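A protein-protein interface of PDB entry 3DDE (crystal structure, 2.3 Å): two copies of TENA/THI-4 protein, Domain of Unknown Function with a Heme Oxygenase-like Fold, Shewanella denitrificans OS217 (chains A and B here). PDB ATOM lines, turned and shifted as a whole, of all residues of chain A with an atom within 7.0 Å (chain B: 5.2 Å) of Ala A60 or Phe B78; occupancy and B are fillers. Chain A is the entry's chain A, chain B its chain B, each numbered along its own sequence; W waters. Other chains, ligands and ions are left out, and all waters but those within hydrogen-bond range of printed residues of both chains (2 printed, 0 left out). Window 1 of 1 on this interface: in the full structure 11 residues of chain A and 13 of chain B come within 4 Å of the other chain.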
ATOM      1  N   HIS A  54      14.496 -31.818  -3.061  1.00  0.00           N
ATOM      2  CA  HIS A  54      14.798 -31.779  -1.638  1.00  0.00           C
ATOM      3  C   HIS A  54      14.717 -30.403  -0.968  1.00  0.00           C
ATOM      4  O   HIS A  54      14.834 -30.313   0.251  1.00  0.00           O
ATOM      5  CB  HIS A  54      16.201 -32.375  -1.400  1.00  0.00           C
ATOM      6  CG  HIS A  54      16.301 -33.831  -1.734  1.00  0.00           C
ATOM      7  ND1 HIS A  54      15.860 -34.821  -0.881  1.00  0.00           N
ATOM      8  CD2 HIS A  54      16.776 -34.466  -2.833  1.00  0.00           C
ATOM      9  CE1 HIS A  54      16.063 -36.002  -1.435  1.00  0.00           C
ATOM     10  NE2 HIS A  54      16.613 -35.815  -2.622  1.00  0.00           N
ATOM     11  N   ASN A  55      14.489 -29.345  -1.739  1.00  0.00           N
ATOM     12  CA  ASN A  55      14.542 -27.994  -1.177  1.00  0.00           C
ATOM     13  C   ASN A  55      13.464 -27.615  -0.165  1.00  0.00           C
ATOM     14  O   ASN A  55      13.782 -26.966   0.849  1.00  0.00           O
ATOM     15  CB  ASN A  55      14.733 -26.953  -2.287  1.00  0.00           C
ATOM     16  CG  ASN A  55      16.163 -26.935  -2.808  1.00  0.00           C
ATOM     17  OD1 ASN A  55      17.070 -27.616  -2.263  1.00  0.00           O
ATOM     18  ND2 ASN A  55      16.389 -26.159  -3.830  1.00  0.00           N
ATOM     19  N   ALA A  56      12.222 -28.029  -0.423  1.00  0.00           N
ATOM     20  CA  ALA A  56      11.135 -27.803   0.508  1.00  0.00           C
ATOM     21  C   ALA A  56      11.457 -28.500   1.827  1.00  0.00           C
ATOM     22  O   ALA A  56      11.243 -27.953   2.894  1.00  0.00           O
ATOM     23  CB  ALA A  56       9.796 -28.321  -0.065  1.00  0.00           C
ATOM     24  N   LYS A  57      11.980 -29.715   1.721  1.00  0.00           N
ATOM     25  CA  LYS A  57      12.313 -30.546   2.873  1.00  0.00           C
ATOM     26  C   LYS A  57      13.438 -29.970   3.717  1.00  0.00           C
ATOM     27  O   LYS A  57      13.273 -29.852   4.924  1.00  0.00           O
ATOM     28  CB  LYS A  57      12.682 -31.938   2.415  1.00  0.00           C
ATOM     29  CG  LYS A  57      11.541 -32.669   1.770  1.00  0.00           C
ATOM     30  CD  LYS A  57      11.960 -34.076   1.417  1.00  0.00           C
ATOM     31  CE  LYS A  57      10.802 -34.820   0.847  1.00  0.00           C
ATOM     32  NZ  LYS A  57      11.059 -36.274   0.837  1.00  0.00           N
ATOM     33  N   ASN A  58      14.558 -29.592   3.103  1.00  0.00           N
ATOM     34  CA  ASN A  58      15.634 -29.019   3.884  1.00  0.00           C
ATOM     35  C   ASN A  58      15.306 -27.608   4.440  1.00  0.00           C
ATOM     36  O   ASN A  58      15.820 -27.228   5.499  1.00  0.00           O
ATOM     37  CB  ASN A  58      17.028 -29.166   3.206  1.00  0.00           C
ATOM     38  CG  ASN A  58      17.154 -28.459   1.853  1.00  0.00           C
ATOM     39  OD1 ASN A  58      16.788 -27.282   1.672  1.00  0.00           O
ATOM     40  ND2 ASN A  58      17.754 -29.164   0.921  1.00  0.00           N
ATOM     41  N   GLN A  59      14.418 -26.867   3.763  1.00  0.00           N
ATOM     42  CA  GLN A  59      13.943 -25.586   4.277  1.00  0.00           C
ATOM     43  C   GLN A  59      13.092 -25.814   5.541  1.00  0.00           C
ATOM     44  O   GLN A  59      13.259 -25.118   6.547  1.00  0.00           O
ATOM     45  CB  GLN A  59      13.127 -24.839   3.215  1.00  0.00           C
ATOM     46  CG  GLN A  59      12.524 -23.515   3.663  1.00  0.00           C
ATOM     47  CD  GLN A  59      13.561 -22.537   4.199  1.00  0.00           C
ATOM     48  OE1 GLN A  59      14.078 -21.697   3.456  1.00  0.00           O
ATOM     49  NE2 GLN A  59      13.914 -22.679   5.480  1.00  0.00           N
ATOM     50  N   ALA A  60      12.185 -26.781   5.489  1.00  0.00           N
ATOM     51  CA  ALA A  60      11.359 -27.103   6.651  1.00  0.00           C
ATOM     52  C   ALA A  60      12.236 -27.587   7.819  1.00  0.00           C
ATOM     53  O   ALA A  60      11.932 -27.336   8.979  1.00  0.00           O
ATOM     54  CB  ALA A  60      10.269 -28.157   6.295  1.00  0.00           C
ATOM     55  N   LEU A  61      13.344 -28.245   7.503  1.00  0.00           N
ATOM     56  CA  LEU A  61      14.248 -28.780   8.524  1.00  0.00           C
ATOM     57  C   LEU A  61      14.883 -27.698   9.420  1.00  0.00           C
ATOM     58  O   LEU A  61      15.086 -27.923  10.621  1.00  0.00           O
ATOM     59  CB  LEU A  61      15.311 -29.655   7.852  1.00  0.00           C
ATOM     60  CG  LEU A  61      16.164 -30.591   8.706  1.00  0.00           C
ATOM     61  CD1 LEU A  61      15.306 -31.505   9.604  1.00  0.00           C
ATOM     62  CD2 LEU A  61      17.062 -31.403   7.773  1.00  0.00           C
ATOM     63  N   VAL A  62      15.190 -26.529   8.849  1.00  0.00           N
ATOM     64  CA  VAL A  62      15.715 -25.409   9.636  1.00  0.00           C
ATOM     65  C   VAL A  62      14.753 -25.095  10.804  1.00  0.00           C
ATOM     66  O   VAL A  62      15.189 -24.843  11.941  1.00  0.00           O
ATOM     67  CB  VAL A  62      15.871 -24.117   8.782  1.00  0.00           C
ATOM     68  CG1 VAL A  62      16.399 -22.933   9.647  1.00  0.00           C
ATOM     69  CG2 VAL A  62      16.755 -24.357   7.527  1.00  0.00           C
ATOM     70  N   GLY A  63      13.451 -25.098  10.514  1.00  0.00           N
ATOM     71  CA  GLY A  63      12.423 -24.803  11.522  1.00  0.00           C
ATOM     72  C   GLY A  63      12.252 -25.871  12.590  1.00  0.00           C
ATOM     73  O   GLY A  63      11.862 -25.585  13.709  1.00  0.00           O
ATOM     74  N   ILE A  64      12.553 -27.114  12.241  1.00  0.00           N
ATOM     75  CA  ILE A  64      12.481 -28.214  13.183  1.00  0.00           C
ATOM     76  C   ILE A  64      13.725 -28.296  14.067  1.00  0.00           C
ATOM     77  O   ILE A  64      13.602 -28.547  15.257  1.00  0.00           O
ATOM     78  CB  ILE A  64      12.276 -29.554  12.439  1.00  0.00           C
ATOM     79  CG1 ILE A  64      10.940 -29.516  11.694  1.00  0.00           C
ATOM     80  CG2 ILE A  64      12.310 -30.726  13.418  1.00  0.00           C
ATOM     81  CD1 ILE A  64      10.937 -30.381  10.476  1.00  0.00           C
ATOM     82  N   MET A  65      14.909 -28.087  13.482  1.00  0.00           N
ATOM     83  CA  MET A  65      16.196 -28.217  14.198  1.00  0.00           C
ATOM     84  C   MET A  65      16.705 -26.943  14.864  1.00  0.00           C
ATOM     85  O   MET A  65      17.455 -27.023  15.842  1.00  0.00           O
ATOM     86  CB  MET A  65      17.288 -28.691  13.246  1.00  0.00           C
ATOM     87  CG  MET A  65      17.006 -30.007  12.627  1.00  0.00           C
ATOM     88  SD  MET A  65      16.806 -31.417  13.876  1.00  0.00           S
ATOM     89  CE  MET A  65      18.677 -31.583  14.417  1.00  0.00           C
ATOM     90  N   LEU A  74      10.620 -18.859  12.083  1.00  0.00           N
ATOM     91  CA  LEU A  74      10.012 -20.196  12.081  1.00  0.00           C
ATOM     92  C   LEU A  74       8.872 -20.229  11.060  1.00  0.00           C
ATOM     93  O   LEU A  74       8.764 -21.184  10.292  1.00  0.00           O
ATOM     94  CB  LEU A  74       9.475 -20.580  13.467  1.00  0.00           C
ATOM     95  CG  LEU A  74       8.762 -21.935  13.612  1.00  0.00           C
ATOM     96  CD1 LEU A  74       9.755 -23.111  13.506  1.00  0.00           C
ATOM     97  CD2 LEU A  74       8.021 -21.970  14.927  1.00  0.00           C
ATOM     98  N   CYS A  77      10.254 -20.391   7.477  1.00  0.00           N
ATOM     99  CA  CYS A  77      10.725 -21.722   7.079  1.00  0.00           C
ATOM    100  C   CYS A  77       9.615 -22.638   6.592  1.00  0.00           C
ATOM    101  O   CYS A  77       9.765 -23.290   5.560  1.00  0.00           O
ATOM    102  CB  CYS A  77      11.455 -22.411   8.226  1.00  0.00           C
ATOM    103  SG  CYS A  77      13.003 -21.632   8.610  1.00  0.00           S
ATOM    104  N   PHE A  78       8.509 -22.701   7.334  1.00  0.00           N
ATOM    105  CA  PHE A  78       7.407 -23.576   6.945  1.00  0.00           C
ATOM    106  C   PHE A  78       6.633 -23.002   5.778  1.00  0.00           C
ATOM    107  O   PHE A  78       6.188 -23.742   4.895  1.00  0.00           O
ATOM    108  CB  PHE A  78       6.488 -23.919   8.124  1.00  0.00           C
ATOM    109  CG  PHE A  78       7.195 -24.628   9.263  1.00  0.00           C
ATOM    110  CD1 PHE A  78       8.176 -25.582   9.022  1.00  0.00           C
ATOM    111  CD2 PHE A  78       6.842 -24.374  10.572  1.00  0.00           C
ATOM    112  CE1 PHE A  78       8.804 -26.239  10.087  1.00  0.00           C
ATOM    113  CE2 PHE A  78       7.467 -25.030  11.622  1.00  0.00           C
ATOM    114  CZ  PHE A  78       8.424 -25.959  11.384  1.00  0.00           C
ATOM    115  N   HIS A  79       6.477 -21.683   5.759  1.00  0.00           N
ATOM    116  CA  HIS A  79       5.796 -21.046   4.649  1.00  0.00           C
ATOM    117  C   HIS A  79       6.517 -21.319   3.348  1.00  0.00           C
ATOM    118  O   HIS A  79       5.891 -21.726   2.368  1.00  0.00           O
ATOM    119  CB  HIS A  79       5.694 -19.534   4.822  1.00  0.00           C
ATOM    120  CG  HIS A  79       5.243 -18.831   3.576  1.00  0.00           C
ATOM    121  ND1 HIS A  79       3.978 -18.982   3.057  1.00  0.00           N
ATOM    122  CD2 HIS A  79       5.902 -18.003   2.731  1.00  0.00           C
ATOM    123  CE1 HIS A  79       3.869 -18.265   1.952  1.00  0.00           C
ATOM    124  NE2 HIS A  79       5.025 -17.667   1.728  1.00  0.00           N
ATOM    125  N   HIS A  80       7.822 -21.072   3.327  1.00  0.00           N
ATOM    126  CA  HIS A  80       8.591 -21.298   2.112  1.00  0.00           C
ATOM    127  C   HIS A  80       8.737 -22.746   1.714  1.00  0.00           C
ATOM    128  O   HIS A  80       8.813 -23.035   0.520  1.00  0.00           O
ATOM    129  CB  HIS A  80       9.917 -20.535   2.115  1.00  0.00           C
ATOM    130  CG  HIS A  80       9.734 -19.102   1.768  1.00  0.00           C
ATOM    131  ND1 HIS A  80       9.718 -18.663   0.463  1.00  0.00           N
ATOM    132  CD2 HIS A  80       9.413 -18.029   2.530  1.00  0.00           C
ATOM    133  CE1 HIS A  80       9.453 -17.370   0.441  1.00  0.00           C
ATOM    134  NE2 HIS A  80       9.257 -16.962   1.682  1.00  0.00           N
ATOM    135  N   ALA A  81       8.753 -23.652   2.689  1.00  0.00           N
ATOM    136  CA  ALA A  81       8.786 -25.093   2.408  1.00  0.00           C
ATOM    137  C   ALA A  81       7.475 -25.431   1.673  1.00  0.00           C
ATOM    138  O   ALA A  81       7.463 -26.183   0.697  1.00  0.00           O
ATOM    139  CB  ALA A  81       8.913 -25.914   3.721  1.00  0.00           C
ATOM    140  N   HIS A  82       6.375 -24.863   2.150  1.00  0.00           N
ATOM    141  CA  HIS A  82       5.075 -25.072   1.510  1.00  0.00           C
ATOM    142  C   HIS A  82       5.053 -24.532   0.074  1.00  0.00           C
ATOM    143  O   HIS A  82       4.516 -25.178  -0.830  1.00  0.00           O
ATOM    144  CB  HIS A  82       3.980 -24.412   2.336  1.00  0.00           C
ATOM    145  CG  HIS A  82       2.628 -24.437   1.698  1.00  0.00           C
ATOM    146  ND1 HIS A  82       1.941 -23.289   1.382  1.00  0.00           N
ATOM    147  CD2 HIS A  82       1.838 -25.469   1.318  1.00  0.00           C
ATOM    148  CE1 HIS A  82       0.769 -23.613   0.861  1.00  0.00           C
ATOM    149  NE2 HIS A  82       0.685 -24.930   0.802  1.00  0.00           N
ATOM    150  N   GLU A  83       5.635 -23.349  -0.124  1.00  0.00           N
ATOM    151  CA  GLU A  83       5.709 -22.730  -1.455  1.00  0.00           C
ATOM    152  C   GLU A  83       6.586 -23.523  -2.425  1.00  0.00           C
ATOM    153  O   GLU A  83       6.258 -23.621  -3.612  1.00  0.00           O
ATOM    154  CB  GLU A  83       6.178 -21.269  -1.373  1.00  0.00           C
ATOM    155  CG  GLU A  83       5.144 -20.351  -0.772  1.00  0.00           C
ATOM    156  CD  GLU A  83       3.834 -20.415  -1.534  1.00  0.00           C
ATOM    157  OE1 GLU A  83       3.808 -20.001  -2.721  1.00  0.00           O
ATOM    158  OE2 GLU A  83       2.827 -20.878  -0.940  1.00  0.00           O
ATOM    159  N   GLU A  84       7.680 -24.103  -1.920  1.00  0.00           N
ATOM    160  CA  GLU A  84       8.572 -24.911  -2.752  1.00  0.00           C
ATOM    161  C   GLU A  84       8.080 -26.324  -3.048  1.00  0.00           C
ATOM    162  O   GLU A  84       8.538 -26.934  -3.995  1.00  0.00           O
ATOM    163  CB  GLU A  84       9.956 -25.037  -2.105  1.00  0.00           C
ATOM    164  CG  GLU A  84      10.694 -23.736  -2.027  1.00  0.00           C
ATOM    165  CD  GLU A  84      10.915 -23.129  -3.398  1.00  0.00           C
ATOM    166  OE1 GLU A  84      11.757 -23.673  -4.146  1.00  0.00           O
ATOM    167  OE2 GLU A  84      10.249 -22.117  -3.716  1.00  0.00           O
ATOM    168  N   ALA A  85       7.180 -26.862  -2.234  1.00  0.00           N
ATOM    169  CA  ALA A  85       6.749 -28.254  -2.418  1.00  0.00           C
ATOM    170  C   ALA A  85       6.240 -28.531  -3.839  1.00  0.00           C
ATOM    171  O   ALA A  85       5.378 -27.813  -4.363  1.00  0.00           O
ATOM    172  CB  ALA A  85       5.719 -28.674  -1.371  1.00  0.00           C
ATOM    173  N   SER A 125      21.223 -27.070   6.995  1.00  0.00           N
ATOM    174  CA  SER A 125      19.856 -26.851   7.434  1.00  0.00           C
ATOM    175  C   SER A 125      19.579 -27.526   8.782  1.00  0.00           C
ATOM    176  O   SER A 125      18.788 -27.032   9.577  1.00  0.00           O
ATOM    177  CB  SER A 125      18.880 -27.358   6.374  1.00  0.00           C
ATOM    178  OG  SER A 125      19.053 -26.649   5.158  1.00  0.00           O
ATOM    179  N   ARG A 133      21.101 -21.003   6.032  1.00  0.00           N
ATOM    180  CA  ARG A 133      20.490 -21.446   4.785  1.00  0.00           C
ATOM    181  C   ARG A 133      19.971 -20.254   3.953  1.00  0.00           C
ATOM    182  O   ARG A 133      19.836 -20.364   2.735  1.00  0.00           O
ATOM    183  CB  ARG A 133      19.357 -22.442   5.045  1.00  0.00           C
ATOM    184  CG  ARG A 133      18.903 -23.184   3.804  1.00  0.00           C
ATOM    185  CD  ARG A 133      17.540 -23.816   3.975  1.00  0.00           C
ATOM    186  NE  ARG A 133      17.132 -24.508   2.751  1.00  0.00           N
ATOM    187  CZ  ARG A 133      16.604 -23.921   1.684  1.00  0.00           C
ATOM    188  NH1 ARG A 133      16.432 -22.601   1.632  1.00  0.00           N
ATOM    189  NH2 ARG A 133      16.282 -24.657   0.633  1.00  0.00           N
ATOM    190  N   ALA B  60       5.652 -30.731  10.353  1.00  0.00           N
ATOM    191  CA  ALA B  60       6.585 -30.519   9.250  1.00  0.00           C
ATOM    192  C   ALA B  60       7.455 -31.767   9.031  1.00  0.00           C
ATOM    193  O   ALA B  60       7.769 -32.121   7.891  1.00  0.00           O
ATOM    194  CB  ALA B  60       7.457 -29.254   9.494  1.00  0.00           C
ATOM    195  N   GLY B  63       6.540 -34.527   6.557  1.00  0.00           N
ATOM    196  CA  GLY B  63       6.844 -34.161   5.177  1.00  0.00           C
ATOM    197  C   GLY B  63       8.282 -34.385   4.779  1.00  0.00           C
ATOM    198  O   GLY B  63       8.583 -34.603   3.601  1.00  0.00           O
ATOM    199  N   ILE B  64       9.169 -34.296   5.761  1.00  0.00           N
ATOM    200  CA  ILE B  64      10.586 -34.504   5.565  1.00  0.00           C
ATOM    201  C   ILE B  64      10.979 -35.977   5.588  1.00  0.00           C
ATOM    202  O   ILE B  64      11.843 -36.397   4.823  1.00  0.00           O
ATOM    203  CB  ILE B  64      11.390 -33.799   6.687  1.00  0.00           C
ATOM    204  CG1 ILE B  64      11.315 -32.279   6.519  1.00  0.00           C
ATOM    205  CG2 ILE B  64      12.858 -34.279   6.701  1.00  0.00           C
ATOM    206  CD1 ILE B  64      11.764 -31.538   7.782  1.00  0.00           C
ATOM    207  N   LEU B  74       2.139 -33.939   1.063  1.00  0.00           N
ATOM    208  CA  LEU B  74       3.385 -33.210   1.368  1.00  0.00           C
ATOM    209  C   LEU B  74       3.039 -31.728   1.545  1.00  0.00           C
ATOM    210  O   LEU B  74       3.500 -31.097   2.492  1.00  0.00           O
ATOM    211  CB  LEU B  74       4.432 -33.389   0.252  1.00  0.00           C
ATOM    212  CG  LEU B  74       5.789 -32.674   0.422  1.00  0.00           C
ATOM    213  CD1 LEU B  74       6.548 -33.193   1.641  1.00  0.00           C
ATOM    214  CD2 LEU B  74       6.648 -32.809  -0.817  1.00  0.00           C
ATOM    215  N   SER B  75       2.220 -31.188   0.642  1.00  0.00           N
ATOM    216  CA  SER B  75       1.785 -29.792   0.737  1.00  0.00           C
ATOM    217  C   SER B  75       1.049 -29.561   2.052  1.00  0.00           C
ATOM    218  O   SER B  75       1.295 -28.580   2.748  1.00  0.00           O
ATOM    219  CB  SER B  75       0.882 -29.429  -0.433  1.00  0.00           C
ATOM    220  OG  SER B  75       1.520 -29.699  -1.666  1.00  0.00           O
ATOM    221  N   PHE B  76       0.143 -30.474   2.366  1.00  0.00           N
ATOM    222  CA  PHE B  76      -0.618 -30.436   3.594  1.00  0.00           C
ATOM    223  C   PHE B  76       0.272 -30.330   4.846  1.00  0.00           C
ATOM    224  O   PHE B  76       0.032 -29.514   5.734  1.00  0.00           O
ATOM    225  CB  PHE B  76      -1.461 -31.700   3.658  1.00  0.00           C
ATOM    226  CG  PHE B  76      -2.220 -31.842   4.922  1.00  0.00           C
ATOM    227  CD1 PHE B  76      -1.621 -32.411   6.041  1.00  0.00           C
ATOM    228  CD2 PHE B  76      -3.540 -31.409   5.001  1.00  0.00           C
ATOM    229  CE1 PHE B  76      -2.312 -32.532   7.228  1.00  0.00           C
ATOM    230  CE2 PHE B  76      -4.248 -31.543   6.176  1.00  0.00           C
ATOM    231  CZ  PHE B  76      -3.636 -32.105   7.296  1.00  0.00           C
ATOM    232  N   CYS B  77       1.295 -31.176   4.928  1.00  0.00           N
ATOM    233  CA  CYS B  77       2.197 -31.165   6.077  1.00  0.00           C
ATOM    234  C   CYS B  77       2.872 -29.810   6.312  1.00  0.00           C
ATOM    235  O   CYS B  77       2.957 -29.356   7.454  1.00  0.00           O
ATOM    236  CB  CYS B  77       3.283 -32.229   5.926  1.00  0.00           C
ATOM    237  SG  CYS B  77       2.675 -33.920   5.909  1.00  0.00           S
ATOM    238  N   PHE B  78       3.373 -29.186   5.241  1.00  0.00           N
ATOM    239  CA  PHE B  78       4.075 -27.912   5.374  1.00  0.00           C
ATOM    240  C   PHE B  78       3.101 -26.756   5.545  1.00  0.00           C
ATOM    241  O   PHE B  78       3.410 -25.806   6.248  1.00  0.00           O
ATOM    242  CB  PHE B  78       5.049 -27.645   4.210  1.00  0.00           C
ATOM    243  CG  PHE B  78       6.151 -28.701   4.041  1.00  0.00           C
ATOM    244  CD1 PHE B  78       6.846 -29.221   5.133  1.00  0.00           C
ATOM    245  CD2 PHE B  78       6.549 -29.102   2.773  1.00  0.00           C
ATOM    246  CE1 PHE B  78       7.853 -30.173   4.949  1.00  0.00           C
ATOM    247  CE2 PHE B  78       7.570 -30.037   2.600  1.00  0.00           C
ATOM    248  CZ  PHE B  78       8.223 -30.560   3.689  1.00  0.00           C
ATOM    249  N   HIS B  79       1.936 -26.838   4.917  1.00  0.00           N
ATOM    250  CA  HIS B  79       0.913 -25.814   5.081  1.00  0.00           C
ATOM    251  C   HIS B  79       0.443 -25.773   6.527  1.00  0.00           C
ATOM    252  O   HIS B  79       0.462 -24.723   7.167  1.00  0.00           O
ATOM    253  CB  HIS B  79      -0.265 -26.041   4.110  1.00  0.00           C
ATOM    254  CG  HIS B  79      -1.437 -25.142   4.360  1.00  0.00           C
ATOM    255  ND1 HIS B  79      -1.364 -23.771   4.241  1.00  0.00           N
ATOM    256  CD2 HIS B  79      -2.717 -25.423   4.704  1.00  0.00           C
ATOM    257  CE1 HIS B  79      -2.547 -23.244   4.508  1.00  0.00           C
ATOM    258  NE2 HIS B  79      -3.382 -24.225   4.806  1.00  0.00           N
ATOM    259  N   HIS B  80       0.056 -26.925   7.046  1.00  0.00           N
ATOM    260  CA  HIS B  80      -0.395 -27.034   8.430  1.00  0.00           C
ATOM    261  C   HIS B  80       0.663 -26.713   9.486  1.00  0.00           C
ATOM    262  O   HIS B  80       0.330 -26.205  10.560  1.00  0.00           O
ATOM    263  CB  HIS B  80      -1.126 -28.363   8.659  1.00  0.00           C
ATOM    264  CG  HIS B  80      -2.497 -28.344   8.068  1.00  0.00           C
ATOM    265  ND1 HIS B  80      -3.613 -28.029   8.813  1.00  0.00           N
ATOM    266  CD2 HIS B  80      -2.910 -28.408   6.782  1.00  0.00           C
ATOM    267  CE1 HIS B  80      -4.667 -27.968   8.020  1.00  0.00           C
ATOM    268  NE2 HIS B  80      -4.269 -28.190   6.779  1.00  0.00           N
ATOM    269  N   ALA B  81       1.926 -26.976   9.177  1.00  0.00           N
ATOM    270  CA  ALA B  81       3.018 -26.629  10.087  1.00  0.00           C
ATOM    271  C   ALA B  81       3.086 -25.109  10.134  1.00  0.00           C
ATOM    272  O   ALA B  81       3.262 -24.510  11.193  1.00  0.00           O
ATOM    273  CB  ALA B  81       4.349 -27.229   9.619  1.00  0.00           C
ATOM    274  N   HIS B  82       2.952 -24.492   8.972  1.00  0.00           N
ATOM    275  CA  HIS B  82       2.927 -23.045   8.885  1.00  0.00           C
ATOM    276  C   HIS B  82       1.730 -22.454   9.654  1.00  0.00           C
ATOM    277  O   HIS B  82       1.874 -21.461  10.350  1.00  0.00           O
ATOM    278  CB  HIS B  82       2.922 -22.616   7.427  1.00  0.00           C
ATOM    279  CG  HIS B  82       2.787 -21.144   7.225  1.00  0.00           C
ATOM    280  ND1 HIS B  82       1.732 -20.583   6.541  1.00  0.00           N
ATOM    281  CD2 HIS B  82       3.573 -20.116   7.621  1.00  0.00           C
ATOM    282  CE1 HIS B  82       1.890 -19.272   6.498  1.00  0.00           C
ATOM    283  NE2 HIS B  82       2.997 -18.962   7.150  1.00  0.00           N
ATOM    284  N   GLU B  83       0.567 -23.077   9.531  1.00  0.00           N
ATOM    285  CA  GLU B  83      -0.654 -22.623  10.227  1.00  0.00           C
ATOM    286  C   GLU B  83      -0.529 -22.736  11.743  1.00  0.00           C
ATOM    287  O   GLU B  83      -1.052 -21.890  12.471  1.00  0.00           O
ATOM    288  CB  GLU B  83      -1.856 -23.469   9.772  1.00  0.00           C
ATOM    289  CG  GLU B  83      -2.260 -23.275   8.319  1.00  0.00           C
ATOM    290  CD  GLU B  83      -3.001 -22.001   8.115  1.00  0.00           C
ATOM    291  OE1 GLU B  83      -4.133 -21.890   8.666  1.00  0.00           O
ATOM    292  OE2 GLU B  83      -2.476 -21.105   7.404  1.00  0.00           O
HETATM  293  O   HOH W   1       8.289 -36.738   1.790  1.00  0.00           O
HETATM  294  O   HOH W   2       1.895 -21.359   3.453  1.00  0.00           O
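A ring nitrogen (ND1) of His A82 sits at hydrogen-bond distance from the side-chain carboxylate of Glu A83 (3.5 Å).
Among the printed residues, pairs that only touch across the chains: Ala A56 with Phe B78 (3.9 Å), Lys A57 with Gly B63 (3.5 Å), Lys A57 with Ile B64 (3.5 Å), Ala A60 with Ile B64 (3.98 Å), Ala A60 with Phe B78 (3.4 Å), Leu A61 with Ile B64 (3.7 Å), Ile A64 with Ala B60 (3.8 Å), Ile A64 with Ile B64 (3.0 Å), Phe A78 with Ala B60 (3.4 Å), Phe A78 with Phe B78 (3.7 Å), Phe A78 with Ala B81 (3.6 Å), Phe A78 with His B82 (3.7 Å), His A79 with His B82 (3.6 Å), Ala A81 with Phe B78 (3.7 Å), His A82 with Ser B75 (3.5 Å), His A82 with Phe B78 (3.7 Å) and His A82 with His B79 (3.5 Å).
Ala A60 touches two residues of chain B. Phe B78 touches just these residues of chain A: Ala A56, Ala A60, Phe A78, Ala A81 and His A82. Printed residues of chain A within 4 Å of Ala B60: Ile A64 (3.8 Å) and Phe A78 (3.4 Å). Of the printed residues of chain B, His A79 touches His B82. Of the printed residues of chain A, His B82 touches Phe A78 and His A79. His B80 touches none of the printed residues of chain A. The nearest residue of chain A that does not touch Phe B78 is Lys A57 (4.2 Å).
Of the 24 printed residues of chain A, 9 touch a printed residue of chain B. Hydrophobic or aromatic side chains of chain A that line the printed part of chain B: Ala A56, Ala A60, Leu A61, Ile A64, Phe A78, His A79, Ala A81 and His A82. Printed residues of chain B that touch a printed residue of chain A: Ala B60, Gly B63, Ile B64, Ser B75, Phe B78, His B79, Ala B81 and His B82.
Ala A60 touches Phe B78, and with the chains exchanged Phe A78 touches Ala B60. Ile A64 touches its own counterpart, Ile B64. Phe A78 touches Ala B81, and with the chains exchanged Ala A81 touches Phe B78. Phe A78 touches His B82, and with the chains exchanged His A82 touches Phe B78. Of the 17 pairs that touch across the chains among the printed residues, 12 have their exchanged pair printed and touching as well.
Water W1 bridges the backbone carbonyl oxygen of Gly B63 (2.8 Å) and the side-chain amino group of Lys A57 (3.0 Å). Water W2 lies within hydrogen-bond range of a ring nitrogen (ND1) of His A82 (2.8 Å), a ring nitrogen (ND1) of His A79 (3.2 Å) and a ring nitrogen (ND1) of His B82 (3.2 Å).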
